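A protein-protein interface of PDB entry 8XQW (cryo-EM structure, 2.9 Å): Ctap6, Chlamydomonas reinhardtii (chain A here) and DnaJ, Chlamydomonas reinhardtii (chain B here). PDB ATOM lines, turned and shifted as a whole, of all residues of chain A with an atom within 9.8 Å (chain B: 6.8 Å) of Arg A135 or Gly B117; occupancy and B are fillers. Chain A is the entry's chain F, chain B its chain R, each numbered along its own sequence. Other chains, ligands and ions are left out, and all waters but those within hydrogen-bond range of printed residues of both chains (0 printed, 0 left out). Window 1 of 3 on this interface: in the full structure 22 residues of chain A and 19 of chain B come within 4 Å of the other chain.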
ATOM      1  N   GLN A 132      -2.756  19.228 -32.123  1.00  0.00           N
ATOM      2  CA  GLN A 132      -1.708  19.401 -31.131  1.00  0.00           C
ATOM      3  C   GLN A 132      -0.452  19.964 -31.778  1.00  0.00           C
ATOM      4  O   GLN A 132      -0.410  20.228 -32.978  1.00  0.00           O
ATOM      5  CB  GLN A 132      -1.421  18.079 -30.422  1.00  0.00           C
ATOM      6  CG  GLN A 132      -2.564  17.623 -29.561  1.00  0.00           C
ATOM      7  CD  GLN A 132      -2.184  16.525 -28.623  1.00  0.00           C
ATOM      8  OE1 GLN A 132      -2.492  16.579 -27.443  1.00  0.00           O
ATOM      9  NE2 GLN A 132      -1.501  15.523 -29.135  1.00  0.00           N
ATOM     10  N   ALA A 133       0.581  20.150 -30.965  1.00  0.00           N
ATOM     11  CA  ALA A 133       1.825  20.767 -31.397  1.00  0.00           C
ATOM     12  C   ALA A 133       2.953  20.244 -30.520  1.00  0.00           C
ATOM     13  O   ALA A 133       2.706  19.771 -29.406  1.00  0.00           O
ATOM     14  CB  ALA A 133       1.734  22.295 -31.332  1.00  0.00           C
ATOM     15  N   PRO A 134       4.202  20.319 -30.989  1.00  0.00           N
ATOM     16  CA  PRO A 134       5.259  19.492 -30.388  1.00  0.00           C
ATOM     17  C   PRO A 134       5.808  19.940 -29.035  1.00  0.00           C
ATOM     18  O   PRO A 134       6.351  19.085 -28.327  1.00  0.00           O
ATOM     19  CB  PRO A 134       6.351  19.518 -31.460  1.00  0.00           C
ATOM     20  CG  PRO A 134       5.615  19.709 -32.708  1.00  0.00           C
ATOM     21  CD  PRO A 134       4.554  20.693 -32.364  1.00  0.00           C
ATOM     22  N   ARG A 135       5.721  21.216 -28.649  1.00  0.00           N
ATOM     23  CA  ARG A 135       6.292  21.650 -27.369  1.00  0.00           C
ATOM     24  C   ARG A 135       7.800  21.436 -27.255  1.00  0.00           C
ATOM     25  O   ARG A 135       8.250  20.443 -26.680  1.00  0.00           O
ATOM     26  CB  ARG A 135       5.616  20.977 -26.173  1.00  0.00           C
ATOM     27  CG  ARG A 135       6.187  21.471 -24.848  1.00  0.00           C
ATOM     28  CD  ARG A 135       5.563  20.808 -23.660  1.00  0.00           C
ATOM     29  NE  ARG A 135       4.460  21.598 -23.148  1.00  0.00           N
ATOM     30  CZ  ARG A 135       3.489  21.103 -22.402  1.00  0.00           C
ATOM     31  NH1 ARG A 135       3.489  19.824 -22.086  1.00  0.00           N
ATOM     32  NH2 ARG A 135       2.514  21.883 -21.981  1.00  0.00           N
ATOM     33  N   ALA A 136       8.583  22.321 -27.867  1.00  0.00           N
ATOM     34  CA  ALA A 136      10.044  22.260 -27.882  1.00  0.00           C
ATOM     35  C   ALA A 136      10.681  21.884 -26.548  1.00  0.00           C
ATOM     36  O   ALA A 136      10.126  22.143 -25.480  1.00  0.00           O
ATOM     37  CB  ALA A 136      10.610  23.602 -28.336  1.00  0.00           C
ATOM     38  N   VAL A 137      11.860  21.265 -26.622  1.00  0.00           N
ATOM     39  CA  VAL A 137      12.460  20.579 -25.482  1.00  0.00           C
ATOM     40  C   VAL A 137      12.988  21.542 -24.429  1.00  0.00           C
ATOM     41  O   VAL A 137      13.064  21.185 -23.252  1.00  0.00           O
ATOM     42  CB  VAL A 137      13.581  19.653 -25.973  1.00  0.00           C
ATOM     43  CG1 VAL A 137      12.997  18.391 -26.568  1.00  0.00           C
ATOM     44  CG2 VAL A 137      14.433  20.374 -26.990  1.00  0.00           C
ATOM     45  N   THR A 138      13.392  22.747 -24.819  1.00  0.00           N
ATOM     46  CA  THR A 138      13.929  23.678 -23.835  1.00  0.00           C
ATOM     47  C   THR A 138      12.874  24.168 -22.863  1.00  0.00           C
ATOM     48  O   THR A 138      13.221  24.564 -21.748  1.00  0.00           O
ATOM     49  CB  THR A 138      14.541  24.892 -24.519  1.00  0.00           C
ATOM     50  OG1 THR A 138      13.553  25.923 -24.597  1.00  0.00           O
ATOM     51  CG2 THR A 138      14.977  24.536 -25.916  1.00  0.00           C
ATOM     52  N   ALA A 139      11.602  24.143 -23.259  1.00  0.00           N
ATOM     53  CA  ALA A 139      10.513  24.719 -22.488  1.00  0.00           C
ATOM     54  C   ALA A 139       9.768  23.677 -21.676  1.00  0.00           C
ATOM     55  O   ALA A 139       8.543  23.753 -21.542  1.00  0.00           O
ATOM     56  CB  ALA A 139       9.545  25.457 -23.409  1.00  0.00           C
ATOM     57  N   SER A 140      10.478  22.695 -21.143  1.00  0.00           N
ATOM     58  CA  SER A 140       9.912  21.761 -20.189  1.00  0.00           C
ATOM     59  C   SER A 140      10.618  21.934 -18.858  1.00  0.00           C
ATOM     60  O   SER A 140      11.789  22.314 -18.807  1.00  0.00           O
ATOM     61  CB  SER A 140      10.047  20.322 -20.663  1.00  0.00           C
ATOM     62  OG  SER A 140      10.198  19.448 -19.564  1.00  0.00           O
ATOM     63  N   ALA A 141       9.905  21.640 -17.779  1.00  0.00           N
ATOM     64  CA  ALA A 141      10.415  21.869 -16.439  1.00  0.00           C
ATOM     65  C   ALA A 141      10.700  20.596 -15.665  1.00  0.00           C
ATOM     66  O   ALA A 141      11.010  20.678 -14.475  1.00  0.00           O
ATOM     67  CB  ALA A 141       9.429  22.722 -15.639  1.00  0.00           C
ATOM     68  N   ALA A 142      10.617  19.430 -16.294  1.00  0.00           N
ATOM     69  CA  ALA A 142      10.724  18.176 -15.563  1.00  0.00           C
ATOM     70  C   ALA A 142      12.156  17.739 -15.304  1.00  0.00           C
ATOM     71  O   ALA A 142      12.354  16.694 -14.680  1.00  0.00           O
ATOM     72  CB  ALA A 142       9.986  17.071 -16.313  1.00  0.00           C
ATOM     73  N   PRO A 154      13.621  12.141 -22.303  1.00  0.00           N
ATOM     74  CA  PRO A 154      12.962  11.561 -23.476  1.00  0.00           C
ATOM     75  C   PRO A 154      12.285  12.562 -24.397  1.00  0.00           C
ATOM     76  O   PRO A 154      12.788  12.809 -25.497  1.00  0.00           O
ATOM     77  CB  PRO A 154      11.928  10.618 -22.850  1.00  0.00           C
ATOM     78  CG  PRO A 154      11.725  11.136 -21.480  1.00  0.00           C
ATOM     79  CD  PRO A 154      13.057  11.622 -21.051  1.00  0.00           C
ATOM     80  N   GLN A 155      11.190  13.174 -23.953  1.00  0.00           N
ATOM     81  CA  GLN A 155      10.443  14.118 -24.776  1.00  0.00           C
ATOM     82  C   GLN A 155       9.294  14.708 -23.974  1.00  0.00           C
ATOM     83  O   GLN A 155       8.586  13.971 -23.279  1.00  0.00           O
ATOM     84  CB  GLN A 155       9.903  13.443 -26.036  1.00  0.00           C
ATOM     85  CG  GLN A 155       9.566  14.394 -27.165  1.00  0.00           C
ATOM     86  CD  GLN A 155      10.787  15.062 -27.756  1.00  0.00           C
ATOM     87  OE1 GLN A 155      11.902  14.573 -27.621  1.00  0.00           O
ATOM     88  NE2 GLN A 155      10.577  16.186 -28.422  1.00  0.00           N
ATOM     89  N   PRO A 156       9.045  16.013 -24.066  1.00  0.00           N
ATOM     90  CA  PRO A 156       7.909  16.580 -23.357  1.00  0.00           C
ATOM     91  C   PRO A 156       6.610  16.186 -24.030  1.00  0.00           C
ATOM     92  O   PRO A 156       6.584  15.903 -25.240  1.00  0.00           O
ATOM     93  CB  PRO A 156       8.153  18.096 -23.458  1.00  0.00           C
ATOM     94  CG  PRO A 156       9.576  18.233 -23.840  1.00  0.00           C
ATOM     95  CD  PRO A 156       9.883  17.051 -24.674  1.00  0.00           C
ATOM     96  N   PRO A 157       5.511  16.137 -23.290  1.00  0.00           N
ATOM     97  CA  PRO A 157       4.210  15.909 -23.906  1.00  0.00           C
ATOM     98  C   PRO A 157       3.886  17.003 -24.903  1.00  0.00           C
ATOM     99  O   PRO A 157       4.485  18.085 -24.864  1.00  0.00           O
ATOM    100  CB  PRO A 157       3.250  15.940 -22.713  1.00  0.00           C
ATOM    101  CG  PRO A 157       4.082  15.532 -21.575  1.00  0.00           C
ATOM    102  CD  PRO A 157       5.443  16.087 -21.825  1.00  0.00           C
ATOM    103  N   PRO A 158       2.957  16.764 -25.820  1.00  0.00           N
ATOM    104  CA  PRO A 158       2.618  17.790 -26.801  1.00  0.00           C
ATOM    105  C   PRO A 158       1.585  18.762 -26.257  1.00  0.00           C
ATOM    106  O   PRO A 158       0.818  18.457 -25.343  1.00  0.00           O
ATOM    107  CB  PRO A 158       2.060  16.977 -27.966  1.00  0.00           C
ATOM    108  CG  PRO A 158       1.432  15.827 -27.309  1.00  0.00           C
ATOM    109  CD  PRO A 158       2.264  15.499 -26.102  1.00  0.00           C
ATOM    110  N   LEU A 159       1.573  19.948 -26.843  1.00  0.00           N
ATOM    111  CA  LEU A 159       0.660  21.011 -26.465  1.00  0.00           C
ATOM    112  C   LEU A 159      -0.696  20.797 -27.111  1.00  0.00           C
ATOM    113  O   LEU A 159      -0.870  19.933 -27.965  1.00  0.00           O
ATOM    114  CB  LEU A 159       1.205  22.367 -26.901  1.00  0.00           C
ATOM    115  CG  LEU A 159       2.286  23.005 -26.052  1.00  0.00           C
ATOM    116  CD1 LEU A 159       2.974  24.072 -26.861  1.00  0.00           C
ATOM    117  CD2 LEU A 159       1.657  23.595 -24.816  1.00  0.00           C
ATOM    118  N   ALA A 160      -1.667  21.591 -26.682  1.00  0.00           N
ATOM    119  CA  ALA A 160      -2.869  21.756 -27.476  1.00  0.00           C
ATOM    120  C   ALA A 160      -2.587  22.780 -28.559  1.00  0.00           C
ATOM    121  O   ALA A 160      -1.704  23.624 -28.411  1.00  0.00           O
ATOM    122  CB  ALA A 160      -4.035  22.203 -26.608  1.00  0.00           C
ATOM    123  N   SER A 161      -3.323  22.698 -29.654  1.00  0.00           N
ATOM    124  CA  SER A 161      -3.060  23.543 -30.805  1.00  0.00           C
ATOM    125  C   SER A 161      -3.248  25.008 -30.438  1.00  0.00           C
ATOM    126  O   SER A 161      -4.358  25.405 -30.064  1.00  0.00           O
ATOM    127  CB  SER A 161      -3.995  23.189 -31.950  1.00  0.00           C
ATOM    128  OG  SER A 161      -5.123  24.041 -31.937  1.00  0.00           O
ATOM    129  N   PRO A 162      -2.208  25.835 -30.534  1.00  0.00           N
ATOM    130  CA  PRO A 162      -2.384  27.257 -30.226  1.00  0.00           C
ATOM    131  C   PRO A 162      -3.344  27.958 -31.156  1.00  0.00           C
ATOM    132  O   PRO A 162      -4.025  28.888 -30.719  1.00  0.00           O
ATOM    133  CB  PRO A 162      -0.969  27.824 -30.363  1.00  0.00           C
ATOM    134  CG  PRO A 162      -0.084  26.659 -30.244  1.00  0.00           C
ATOM    135  CD  PRO A 162      -0.813  25.518 -30.852  1.00  0.00           C
ATOM    136  N   LEU A 203      -0.317  13.291 -32.854  1.00  0.00           N
ATOM    137  CA  LEU A 203       0.429  13.956 -33.907  1.00  0.00           C
ATOM    138  C   LEU A 203       0.725  12.999 -35.054  1.00  0.00           C
ATOM    139  O   LEU A 203       0.940  11.804 -34.853  1.00  0.00           O
ATOM    140  CB  LEU A 203       1.726  14.526 -33.348  1.00  0.00           C
ATOM    141  CG  LEU A 203       1.604  15.924 -32.760  1.00  0.00           C
ATOM    142  CD1 LEU A 203       2.673  16.149 -31.736  1.00  0.00           C
ATOM    143  CD2 LEU A 203       1.716  16.944 -33.862  1.00  0.00           C
ATOM    144  N   TYR A 207       5.407  14.790 -38.305  1.00  0.00           N
ATOM    145  CA  TYR A 207       5.510  15.935 -37.421  1.00  0.00           C
ATOM    146  C   TYR A 207       5.899  15.569 -36.001  1.00  0.00           C
ATOM    147  O   TYR A 207       6.269  16.465 -35.237  1.00  0.00           O
ATOM    148  CB  TYR A 207       4.185  16.704 -37.391  1.00  0.00           C
ATOM    149  CG  TYR A 207       3.967  17.553 -38.610  1.00  0.00           C
ATOM    150  CD1 TYR A 207       5.034  18.128 -39.268  1.00  0.00           C
ATOM    151  CD2 TYR A 207       2.701  17.771 -39.107  1.00  0.00           C
ATOM    152  CE1 TYR A 207       4.846  18.902 -40.380  1.00  0.00           C
ATOM    153  CE2 TYR A 207       2.503  18.543 -40.221  1.00  0.00           C
ATOM    154  CZ  TYR A 207       3.581  19.108 -40.852  1.00  0.00           C
ATOM    155  OH  TYR A 207       3.396  19.883 -41.968  1.00  0.00           O
ATOM    156  N   MET A 208       5.819  14.302 -35.621  1.00  0.00           N
ATOM    157  CA  MET A 208       6.329  13.898 -34.323  1.00  0.00           C
ATOM    158  C   MET A 208       7.831  14.149 -34.273  1.00  0.00           C
ATOM    159  O   MET A 208       8.528  13.939 -35.269  1.00  0.00           O
ATOM    160  CB  MET A 208       6.037  12.422 -34.065  1.00  0.00           C
ATOM    161  CG  MET A 208       4.569  12.110 -33.952  1.00  0.00           C
ATOM    162  SD  MET A 208       4.259  10.381 -33.581  1.00  0.00           S
ATOM    163  CE  MET A 208       5.025  10.252 -31.978  1.00  0.00           C
ATOM    164  N   PRO A 209       8.364  14.612 -33.141  1.00  0.00           N
ATOM    165  CA  PRO A 209       9.793  14.934 -33.079  1.00  0.00           C
ATOM    166  C   PRO A 209      10.692  13.724 -32.933  1.00  0.00           C
ATOM    167  O   PRO A 209      11.896  13.846 -33.185  1.00  0.00           O
ATOM    168  CB  PRO A 209       9.896  15.835 -31.842  1.00  0.00           C
ATOM    169  CG  PRO A 209       8.490  16.117 -31.427  1.00  0.00           C
ATOM    170  CD  PRO A 209       7.678  14.973 -31.897  1.00  0.00           C
ATOM    171  N   CYS B 113      -4.824  19.461 -18.040  1.00  0.00           N
ATOM    172  CA  CYS B 113      -4.701  20.630 -18.895  1.00  0.00           C
ATOM    173  C   CYS B 113      -3.526  20.443 -19.838  1.00  0.00           C
ATOM    174  O   CYS B 113      -2.432  20.067 -19.417  1.00  0.00           O
ATOM    175  CB  CYS B 113      -4.522  21.888 -18.051  1.00  0.00           C
ATOM    176  SG  CYS B 113      -5.082  23.427 -18.818  1.00  0.00           S
ATOM    177  N   ARG B 114      -3.764  20.682 -21.122  1.00  0.00           N
ATOM    178  CA  ARG B 114      -2.740  20.547 -22.142  1.00  0.00           C
ATOM    179  C   ARG B 114      -2.038  21.857 -22.438  1.00  0.00           C
ATOM    180  O   ARG B 114      -1.069  21.870 -23.199  1.00  0.00           O
ATOM    181  CB  ARG B 114      -3.350  19.995 -23.427  1.00  0.00           C
ATOM    182  CG  ARG B 114      -3.524  18.501 -23.427  1.00  0.00           C
ATOM    183  CD  ARG B 114      -2.208  17.812 -23.166  1.00  0.00           C
ATOM    184  NE  ARG B 114      -2.139  16.510 -23.815  1.00  0.00           N
ATOM    185  CZ  ARG B 114      -2.741  15.418 -23.361  1.00  0.00           C
ATOM    186  NH1 ARG B 114      -3.461  15.469 -22.250  1.00  0.00           N
ATOM    187  NH2 ARG B 114      -2.624  14.276 -24.017  1.00  0.00           N
ATOM    188  N   VAL B 115      -2.497  22.954 -21.849  1.00  0.00           N
ATOM    189  CA  VAL B 115      -1.969  24.268 -22.159  1.00  0.00           C
ATOM    190  C   VAL B 115      -0.901  24.725 -21.173  1.00  0.00           C
ATOM    191  O   VAL B 115      -0.084  25.584 -21.525  1.00  0.00           O
ATOM    192  CB  VAL B 115      -3.120  25.288 -22.219  1.00  0.00           C
ATOM    193  CG1 VAL B 115      -2.722  26.476 -23.046  1.00  0.00           C
ATOM    194  CG2 VAL B 115      -4.355  24.641 -22.770  1.00  0.00           C
ATOM    195  N   CYS B 116      -0.867  24.179 -19.966  1.00  0.00           N
ATOM    196  CA  CYS B 116      -0.136  24.794 -18.867  1.00  0.00           C
ATOM    197  C   CYS B 116       1.010  23.902 -18.424  1.00  0.00           C
ATOM    198  O   CYS B 116       0.805  22.939 -17.690  1.00  0.00           O
ATOM    199  CB  CYS B 116      -1.085  25.109 -17.707  1.00  0.00           C
ATOM    200  SG  CYS B 116      -1.875  23.728 -16.877  1.00  0.00           S
ATOM    201  N   GLY B 117       2.214  24.218 -18.889  1.00  0.00           N
ATOM    202  CA  GLY B 117       3.436  23.705 -18.299  1.00  0.00           C
ATOM    203  C   GLY B 117       3.557  22.202 -18.204  1.00  0.00           C
ATOM    204  O   GLY B 117       2.679  21.467 -18.649  1.00  0.00           O
ATOM    205  N   THR B 118       4.662  21.728 -17.644  1.00  0.00           N
ATOM    206  CA  THR B 118       4.831  20.325 -17.307  1.00  0.00           C
ATOM    207  C   THR B 118       5.245  20.202 -15.850  1.00  0.00           C
ATOM    208  O   THR B 118       5.915  21.080 -15.307  1.00  0.00           O
ATOM    209  CB  THR B 118       5.878  19.652 -18.189  1.00  0.00           C
ATOM    210  OG1 THR B 118       7.182  20.007 -17.724  1.00  0.00           O
ATOM    211  CG2 THR B 118       5.734  20.088 -19.626  1.00  0.00           C
ATOM    212  N   ALA B 119       4.846  19.103 -15.224  1.00  0.00           N
ATOM    213  CA  ALA B 119       5.153  18.887 -13.820  1.00  0.00           C
ATOM    214  C   ALA B 119       6.660  18.864 -13.590  1.00  0.00           C
ATOM    215  O   ALA B 119       7.455  18.689 -14.513  1.00  0.00           O
ATOM    216  CB  ALA B 119       4.535  17.579 -13.339  1.00  0.00           C
ATOM    217  N   PRO B 299       7.797  27.671 -17.592  1.00  0.00           N
ATOM    218  CA  PRO B 299       6.622  27.549 -16.728  1.00  0.00           C
ATOM    219  C   PRO B 299       6.469  26.148 -16.167  1.00  0.00           C
ATOM    220  O   PRO B 299       7.104  25.200 -16.627  1.00  0.00           O
ATOM    221  CB  PRO B 299       5.465  27.889 -17.665  1.00  0.00           C
ATOM    222  CG  PRO B 299       6.076  28.544 -18.813  1.00  0.00           C
ATOM    223  CD  PRO B 299       7.417  27.973 -18.973  1.00  0.00           C
ATOM    224  N   THR B 300       5.602  26.018 -15.177  1.00  0.00           N
ATOM    225  CA  THR B 300       5.362  24.749 -14.517  1.00  0.00           C
ATOM    226  C   THR B 300       3.889  24.371 -14.621  1.00  0.00           C
ATOM    227  O   THR B 300       3.114  24.994 -15.341  1.00  0.00           O
ATOM    228  CB  THR B 300       5.832  24.814 -13.074  1.00  0.00           C
ATOM    229  OG1 THR B 300       5.553  26.111 -12.547  1.00  0.00           O
ATOM    230  CG2 THR B 300       7.314  24.567 -13.001  1.00  0.00           C
ATOM    231  N   ALA B 301       3.502  23.337 -13.892  1.00  0.00           N
ATOM    232  CA  ALA B 301       2.264  22.625 -14.157  1.00  0.00           C
ATOM    233  C   ALA B 301       1.011  23.425 -13.878  1.00  0.00           C
ATOM    234  O   ALA B 301      -0.078  22.903 -14.113  1.00  0.00           O
ATOM    235  CB  ALA B 301       2.222  21.340 -13.341  1.00  0.00           C
ATOM    236  N   GLY B 302       1.094  24.650 -13.394  1.00  0.00           N
ATOM    237  CA  GLY B 302      -0.138  25.358 -13.128  1.00  0.00           C
ATOM    238  C   GLY B 302      -0.191  26.713 -13.784  1.00  0.00           C
ATOM    239  O   GLY B 302      -1.151  27.459 -13.596  1.00  0.00           O
ATOM    240  N   THR B 303       0.834  27.044 -14.555  1.00  0.00           N
ATOM    241  CA  THR B 303       1.019  28.386 -15.067  1.00  0.00           C
ATOM    242  C   THR B 303       1.356  28.337 -16.544  1.00  0.00           C
ATOM    243  O   THR B 303       1.928  27.369 -17.039  1.00  0.00           O
ATOM    244  CB  THR B 303       2.140  29.107 -14.337  1.00  0.00           C
ATOM    245  OG1 THR B 303       3.392  28.599 -14.793  1.00  0.00           O
ATOM    246  CG2 THR B 303       2.054  28.890 -12.860  1.00  0.00           C
ATOM    247  N   VAL B 304       1.009  29.408 -17.247  1.00  0.00           N
ATOM    248  CA  VAL B 304       1.337  29.573 -18.651  1.00  0.00           C
ATOM    249  C   VAL B 304       2.244  30.785 -18.775  1.00  0.00           C
ATOM    250  O   VAL B 304       2.407  31.554 -17.838  1.00  0.00           O
ATOM    251  CB  VAL B 304       0.089  29.734 -19.526  1.00  0.00           C
ATOM    252  CG1 VAL B 304      -0.983  28.788 -19.072  1.00  0.00           C
ATOM    253  CG2 VAL B 304      -0.417  31.139 -19.453  1.00  0.00           C
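Printed residues of chain B within 4 Å of Gln A132: Arg B114 (3.6 Å).
Arg A135 touches just these residues of chain B: Arg B114 (3.8 Å), Gly B117 (3.4 Å) and Thr B118 (3.3 Å).
Ala A139 touches none of the printed residues of chain B.
Of the printed residues of chain B, Ala A142 touches Thr B118 (3.8 Å) and Ala B119 (3.5 Å).
Pro A162 touches none of the printed residues of chain B.
No residue of chain A comes within 4 Å of Cys B116.
Gly B117 touches just one residue of chain A: Arg A135 (3.4 Å).
Of the printed residues of chain A, Thr B300 touches Ala A141 (3.9 Å).
The nearest residue of chain B that does not touch Arg A135 is Cys B116 (4.4 Å).
The nearest residue of chain A that does not touch Gly B117 is Leu A159 (6.0 Å).
O of Gly B117 lies within hydrogen-bond range of NH2 of Arg A135 (3.4 Å).
OG1 of Thr B118 lies within hydrogen-bond range of N of Ala A141 (3.2 Å).
Printed residues of chain B that touch a printed residue of chain A: Arg B114, Gly B117, Thr B118, Ala B119, Pro B299 and Thr B300.
Of the 24 printed residues of chain A, 8 touch a printed residue of chain B.
Printed residues of chain A that touch a printed residue of chain B: Gln A132, Arg A135, Ser A140, Ala A141, Ala A142, Pro A158, Leu A159 and Ala A160.
Hydrophobic or aromatic side chains of chain A within 4 Å of the printed part of chain B: Ala A141, Ala A142, Leu A159 and Ala A160.
Among the printed residues, 14 pairs touch across the chains.
Among the printed residues, no Asp or Glu carboxylate lies within 4 Å of a Lys or Arg side-chain nitrogen of the other chain.
NE of Arg B114 touches OE1 of Gln A132, 3.6 Å away.
NH2 of Arg A135 touches O of Arg B114 (3.8 Å).
CG2 of Thr B118 touches NH1 of Arg A135, 3.3 Å away.
Thr B118 touches Ser A140 (OG1 to OG, 3.6 Å).
Ala A141 touches Pro B299.
Ala A141 touches Thr B300.
O of Ala B119 touches CA of Ala A142, 3.5 Å away.
O of Pro A158 touches CD of Arg B114, at 3.8 Å.
Arg B114 touches Leu A159 (O to CD2, 3.6 Å).
Arg B114 touches Ala A160.
N of Thr B300 lies within hydrogen-bond range of OG1 of Thr B303 (3.4 Å).
O of Ala A133 is in hydrogen-bond range of N of Leu A159, 2.8 Å away.
NH1 of Arg A135 lies close to O of Pro A157 (3.4 Å).
The side-chain hydroxyl (OG) of Ser A140 sits at hydrogen-bond distance from the backbone NH (N) of Ala A142.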
